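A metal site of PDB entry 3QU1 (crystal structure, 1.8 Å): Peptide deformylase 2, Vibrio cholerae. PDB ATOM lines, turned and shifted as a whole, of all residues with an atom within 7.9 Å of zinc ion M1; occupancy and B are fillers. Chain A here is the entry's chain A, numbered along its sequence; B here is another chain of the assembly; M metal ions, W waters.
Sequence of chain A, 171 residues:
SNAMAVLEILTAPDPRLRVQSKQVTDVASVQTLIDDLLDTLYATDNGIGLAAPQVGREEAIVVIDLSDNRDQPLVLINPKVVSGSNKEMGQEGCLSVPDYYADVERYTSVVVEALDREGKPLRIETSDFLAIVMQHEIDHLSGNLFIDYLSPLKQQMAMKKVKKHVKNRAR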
ATOM      1  N   LEU A  41       5.485 -18.886  15.519  1.00  0.00           N
ATOM      2  CA  LEU A  41       4.234 -18.376  14.962  1.00  0.00           C
ATOM      3  C   LEU A  41       3.680 -17.244  15.823  1.00  0.00           C
ATOM      4  O   LEU A  41       3.265 -16.178  15.279  1.00  0.00           O
ATOM      5  CB  LEU A  41       3.194 -19.467  14.874  1.00  0.00           C
ATOM      6  CG  LEU A  41       1.829 -18.992  14.292  1.00  0.00           C
ATOM      7  CD1 LEU A  41       1.940 -18.507  12.871  1.00  0.00           C
ATOM      8  CD2 LEU A  41       0.835 -20.113  14.439  1.00  0.00           C
ATOM      9  N   GLY A  47       0.863 -13.936  11.758  1.00  0.00           N
ATOM     10  CA  GLY A  47       0.905 -15.202  11.099  1.00  0.00           C
ATOM     11  C   GLY A  47      -0.155 -16.034  11.740  1.00  0.00           C
ATOM     12  O   GLY A  47      -0.441 -15.905  12.954  1.00  0.00           O
ATOM     13  N   ILE A  48      -0.772 -16.858  10.932  1.00  0.00           N
ATOM     14  CA  ILE A  48      -1.763 -17.772  11.421  1.00  0.00           C
ATOM     15  C   ILE A  48      -1.444 -19.209  11.072  1.00  0.00           C
ATOM     16  O   ILE A  48      -2.072 -20.107  11.645  1.00  0.00           O
ATOM     17  CB  ILE A  48      -3.176 -17.404  10.947  1.00  0.00           C
ATOM     18  CG1 ILE A  48      -3.285 -17.466   9.434  1.00  0.00           C
ATOM     19  CG2 ILE A  48      -3.567 -15.969  11.521  1.00  0.00           C
ATOM     20  CD1 ILE A  48      -4.698 -17.098   8.959  1.00  0.00           C
ATOM     21  N   GLY A  49      -0.418 -19.460  10.233  1.00  0.00           N
ATOM     22  CA  GLY A  49       0.019 -20.827   9.956  1.00  0.00           C
ATOM     23  C   GLY A  49       1.479 -20.919   9.658  1.00  0.00           C
ATOM     24  O   GLY A  49       1.999 -20.079   8.974  1.00  0.00           O
ATOM     25  N   LEU A  50       2.170 -21.918  10.198  1.00  0.00           N
ATOM     26  CA  LEU A  50       3.590 -22.100   9.928  1.00  0.00           C
ATOM     27  C   LEU A  50       3.852 -23.577   9.746  1.00  0.00           C
ATOM     28  O   LEU A  50       3.358 -24.391  10.515  1.00  0.00           O
ATOM     29  CB  LEU A  50       4.407 -21.601  11.092  1.00  0.00           C
ATOM     30  CG  LEU A  50       5.922 -21.537  11.062  1.00  0.00           C
ATOM     31  CD1 LEU A  50       6.443 -20.545   9.997  1.00  0.00           C
ATOM     32  CD2 LEU A  50       6.492 -21.171  12.484  1.00  0.00           C
ATOM     33  N   ALA A  51       4.622 -23.916   8.730  1.00  0.00           N
ATOM     34  CA  ALA A  51       4.996 -25.282   8.442  1.00  0.00           C
ATOM     35  C   ALA A  51       6.494 -25.482   8.715  1.00  0.00           C
ATOM     36  O   ALA A  51       7.280 -24.588   8.508  1.00  0.00           O
ATOM     37  CB  ALA A  51       4.687 -25.544   6.988  1.00  0.00           C
ATOM     38  N   GLN A  54       9.559 -24.068   6.822  1.00  0.00           N
ATOM     39  CA  GLN A  54       9.786 -22.635   6.925  1.00  0.00           C
ATOM     40  C   GLN A  54      10.758 -22.277   8.022  1.00  0.00           C
ATOM     41  O   GLN A  54      11.255 -21.152   8.088  1.00  0.00           O
ATOM     42  CB  GLN A  54       8.461 -21.932   7.135  1.00  0.00           C
ATOM     43  CG  GLN A  54       7.481 -22.158   6.047  1.00  0.00           C
ATOM     44  CD  GLN A  54       6.214 -21.356   6.276  1.00  0.00           C
ATOM     45  OE1 GLN A  54       5.197 -21.910   6.748  1.00  0.00           O
ATOM     46  NE2 GLN A  54       6.277 -20.050   5.982  1.00  0.00           N
ATOM     47  N   VAL A  62       2.679 -29.008  10.823  1.00  0.00           N
ATOM     48  CA  VAL A  62       2.142 -27.709  10.566  1.00  0.00           C
ATOM     49  C   VAL A  62       1.498 -27.282  11.909  1.00  0.00           C
ATOM     50  O   VAL A  62       0.875 -28.124  12.591  1.00  0.00           O
ATOM     51  CB  VAL A  62       1.075 -27.823   9.458  1.00  0.00           C
ATOM     52  CG1 VAL A  62      -0.054 -26.757   9.567  1.00  0.00           C
ATOM     53  CG2 VAL A  62       1.769 -27.943   8.035  1.00  0.00           C
ATOM     54  N   VAL A  63       1.606 -25.989  12.224  1.00  0.00           N
ATOM     55  CA  VAL A  63       0.829 -25.384  13.335  1.00  0.00           C
ATOM     56  C   VAL A  63       0.039 -24.189  12.852  1.00  0.00           C
ATOM     57  O   VAL A  63       0.541 -23.435  12.004  1.00  0.00           O
ATOM     58  CB  VAL A  63       1.732 -24.972  14.541  1.00  0.00           C
ATOM     59  CG1 VAL A  63       2.498 -26.214  15.102  1.00  0.00           C
ATOM     60  CG2 VAL A  63       2.706 -23.862  14.216  1.00  0.00           C
ATOM     61  N   ILE A  64      -1.191 -24.078  13.353  1.00  0.00           N
ATOM     62  CA  ILE A  64      -2.171 -23.047  12.943  1.00  0.00           C
ATOM     63  C   ILE A  64      -2.842 -22.476  14.170  1.00  0.00           C
ATOM     64  O   ILE A  64      -3.125 -23.188  15.144  1.00  0.00           O
ATOM     65  CB  ILE A  64      -3.245 -23.653  11.982  1.00  0.00           C
ATOM     66  CG1 ILE A  64      -2.629 -24.035  10.657  1.00  0.00           C
ATOM     67  CG2 ILE A  64      -4.445 -22.695  11.745  1.00  0.00           C
ATOM     68  CD1 ILE A  64      -3.419 -25.057   9.855  1.00  0.00           C
ATOM     69  N   GLY A  93      -1.004 -14.690   1.488  1.00  0.00           N
ATOM     70  CA  GLY A  93       0.385 -14.348   1.687  1.00  0.00           C
ATOM     71  C   GLY A  93       1.109 -15.495   2.319  1.00  0.00           C
ATOM     72  O   GLY A  93       0.558 -16.575   2.431  1.00  0.00           O
ATOM     73  N   CYS A  94       2.364 -15.265   2.698  1.00  0.00           N
ATOM     74  CA  CYS A  94       3.133 -16.312   3.327  1.00  0.00           C
ATOM     75  C   CYS A  94       4.277 -15.699   4.140  1.00  0.00           C
ATOM     76  O   CYS A  94       4.981 -14.855   3.643  1.00  0.00           O
ATOM     77  CB  CYS A  94       3.683 -17.266   2.279  1.00  0.00           C
ATOM     78  SG  CYS A  94       4.682 -18.641   2.918  1.00  0.00           S
ATOM     79  N   LEU A  95       4.489 -16.185   5.358  1.00  0.00           N
ATOM     80  CA  LEU A  95       5.611 -15.708   6.192  1.00  0.00           C
ATOM     81  C   LEU A  95       6.988 -15.896   5.499  1.00  0.00           C
ATOM     82  O   LEU A  95       7.933 -15.133   5.778  1.00  0.00           O
ATOM     83  CB  LEU A  95       5.547 -16.403   7.572  1.00  0.00           C
ATOM     84  CG  LEU A  95       4.304 -16.142   8.403  1.00  0.00           C
ATOM     85  CD1 LEU A  95       4.248 -17.170   9.552  1.00  0.00           C
ATOM     86  CD2 LEU A  95       4.352 -14.709   8.914  1.00  0.00           C
ATOM     87  N   SER A  96       7.089 -16.880   4.598  1.00  0.00           N
ATOM     88  CA  SER A  96       8.345 -17.088   3.875  1.00  0.00           C
ATOM     89  C   SER A  96       8.436 -16.379   2.522  1.00  0.00           C
ATOM     90  O   SER A  96       9.471 -16.465   1.879  1.00  0.00           O
ATOM     91  CB  SER A  96       8.600 -18.581   3.654  1.00  0.00           C
ATOM     92  OG  SER A  96       8.796 -19.252   4.872  1.00  0.00           O
ATOM     93  N   VAL A 133      -6.323 -22.130   4.914  1.00  0.00           N
ATOM     94  CA  VAL A 133      -5.067 -22.115   5.660  1.00  0.00           C
ATOM     95  C   VAL A 133      -4.422 -23.512   5.695  1.00  0.00           C
ATOM     96  O   VAL A 133      -3.198 -23.695   5.543  1.00  0.00           O
ATOM     97  CB  VAL A 133      -5.315 -21.628   7.094  1.00  0.00           C
ATOM     98  CG1 VAL A 133      -4.064 -21.800   7.948  1.00  0.00           C
ATOM     99  CG2 VAL A 133      -5.791 -20.163   7.130  1.00  0.00           C
ATOM    100  N   HIS A 136      -2.768 -24.296   2.319  1.00  0.00           N
ATOM    101  CA  HIS A 136      -1.540 -23.507   2.136  1.00  0.00           C
ATOM    102  C   HIS A 136      -0.413 -24.152   2.950  1.00  0.00           C
ATOM    103  O   HIS A 136       0.684 -24.309   2.494  1.00  0.00           O
ATOM    104  CB  HIS A 136      -1.801 -22.109   2.652  1.00  0.00           C
ATOM    105  CG  HIS A 136      -0.584 -21.245   2.705  1.00  0.00           C
ATOM    106  ND1 HIS A 136      -0.438 -20.125   1.927  1.00  0.00           N
ATOM    107  CD2 HIS A 136       0.551 -21.339   3.449  1.00  0.00           C
ATOM    108  CE1 HIS A 136       0.733 -19.563   2.181  1.00  0.00           C
ATOM    109  NE2 HIS A 136       1.330 -20.265   3.131  1.00  0.00           N
ATOM    110  N   GLU A 137      -0.704 -24.538   4.173  1.00  0.00           N
ATOM    111  CA  GLU A 137       0.358 -25.013   5.055  1.00  0.00           C
ATOM    112  C   GLU A 137       0.806 -26.431   4.703  1.00  0.00           C
ATOM    113  O   GLU A 137       2.020 -26.749   4.701  1.00  0.00           O
ATOM    114  CB  GLU A 137      -0.064 -24.942   6.514  1.00  0.00           C
ATOM    115  CG  GLU A 137      -0.410 -23.571   7.074  1.00  0.00           C
ATOM    116  CD  GLU A 137       0.655 -22.486   6.911  1.00  0.00           C
ATOM    117  OE1 GLU A 137       1.833 -22.806   6.854  1.00  0.00           O
ATOM    118  OE2 GLU A 137       0.259 -21.290   6.862  1.00  0.00           O
ATOM    119  N   HIS A 140       3.302 -26.522   1.911  1.00  0.00           N
ATOM    120  CA  HIS A 140       4.723 -26.335   2.306  1.00  0.00           C
ATOM    121  C   HIS A 140       5.457 -27.692   2.509  1.00  0.00           C
ATOM    122  O   HIS A 140       6.665 -27.800   2.322  1.00  0.00           O
ATOM    123  CB  HIS A 140       4.837 -25.559   3.621  1.00  0.00           C
ATOM    124  CG  HIS A 140       4.688 -24.085   3.479  1.00  0.00           C
ATOM    125  ND1 HIS A 140       5.576 -23.356   2.721  1.00  0.00           N
ATOM    126  CD2 HIS A 140       3.814 -23.197   4.014  1.00  0.00           C
ATOM    127  CE1 HIS A 140       5.232 -22.078   2.791  1.00  0.00           C
ATOM    128  NE2 HIS A 140       4.208 -21.935   3.618  1.00  0.00           N
ATOM    129  N   ARG B 169      -5.609 -12.330   5.158  1.00  0.00           N
ATOM    130  CA  ARG B 169      -5.789 -13.234   6.313  1.00  0.00           C
ATOM    131  C   ARG B 169      -4.734 -14.381   6.290  1.00  0.00           C
ATOM    132  O   ARG B 169      -3.992 -14.625   7.219  1.00  0.00           O
ATOM    133  CB  ARG B 169      -7.207 -13.824   6.251  1.00  0.00           C
ATOM    134  CG  ARG B 169      -8.309 -12.791   6.089  1.00  0.00           C
ATOM    135  CD  ARG B 169      -9.708 -13.410   6.307  1.00  0.00           C
ATOM    136  NE  ARG B 169      -9.811 -13.997   7.644  1.00  0.00           N
ATOM    137  CZ  ARG B 169     -10.835 -14.726   8.057  1.00  0.00           C
ATOM    138  NH1 ARG B 169     -10.842 -15.225   9.300  1.00  0.00           N
ATOM    139  NH2 ARG B 169     -11.855 -14.929   7.247  1.00  0.00           N
ATOM    140  N   ALA B 170      -4.689 -15.098   5.183  1.00  0.00           N
ATOM    141  CA  ALA B 170      -3.795 -16.296   5.127  1.00  0.00           C
ATOM    142  C   ALA B 170      -2.282 -15.905   5.088  1.00  0.00           C
ATOM    143  O   ALA B 170      -1.824 -15.361   4.102  1.00  0.00           O
ATOM    144  CB  ALA B 170      -4.156 -17.160   3.959  1.00  0.00           C
ATOM    145  N   ARG B 171      -1.539 -16.234   6.145  1.00  0.00           N
ATOM    146  CA  ARG B 171      -0.066 -16.114   6.169  1.00  0.00           C
ATOM    147  C   ARG B 171       0.460 -17.369   6.853  1.00  0.00           C
ATOM    148  O   ARG B 171       0.096 -17.609   8.016  1.00  0.00           O
ATOM    149  CB  ARG B 171       0.337 -14.894   6.952  1.00  0.00           C
ATOM    150  CG  ARG B 171       0.162 -13.578   6.197  1.00  0.00           C
ATOM    151  CD  ARG B 171       0.612 -12.446   7.053  1.00  0.00           C
ATOM    152  NE  ARG B 171       0.364 -11.149   6.452  1.00  0.00           N
ATOM    153  CZ  ARG B 171      -0.798 -10.497   6.449  1.00  0.00           C
ATOM    154  NH1 ARG B 171      -1.925 -11.034   7.014  1.00  0.00           N
ATOM    155  NH2 ARG B 171      -0.849  -9.295   5.886  1.00  0.00           N
ATOM    156  OXT ARG B 171       1.177 -18.118   6.255  1.00  0.00           O
HETATM  157 ZN    ZN M   1       1.580 -19.933   6.919  1.00  0.00          ZN
HETATM  158 ZN    ZN M   2       3.277 -20.151   3.909  1.00  0.00          ZN
HETATM  159  O   HOH W   1       3.181 -20.209   5.868  1.00  0.00           O
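The side-chain carboxylate (OE1) of Glu 137 lies within hydrogen-bond range of the backbone NH (N) of Leu 50 (3.5 Å).
The side-chain carboxylate (OE1) of Glu 137 sits close to the side-chain amide oxygen (OE1) of Gln 54 (3.5 Å).
The backbone NH (N) of Ile 48 lies within hydrogen-bond range of the chain-end carboxylate (O) of Arg 171 of chain B (3.1 Å).
N of Leu 50 sits at hydrogen-bond distance from O of Val 63 (2.9 Å).
Leu 50 touches zinc ion M1 (N to ZN, 3.9 Å).
His 136 touches zinc ion M1 (NE2 to ZN, 3.8 Å).
The nearest printed residue that does not touch zinc ion M1 is Gln 54 (4.1 Å).
Zinc ion M1 is bound by the side-chain carboxylate of Glu 137 (1.9 Å), water W1 (1.9 Å), the chain-end carboxylate of Arg 171 of chain B (2.0 Å) and the backbone carbonyl oxygen of Gly 49 (2.1 Å).
Zinc ion M1 has four donor atoms within binding distance.
Water W1 lies within hydrogen-bond range of OE1 of Gln 54 (2.8 Å) and OE1 of Glu 137 (3.1 Å).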
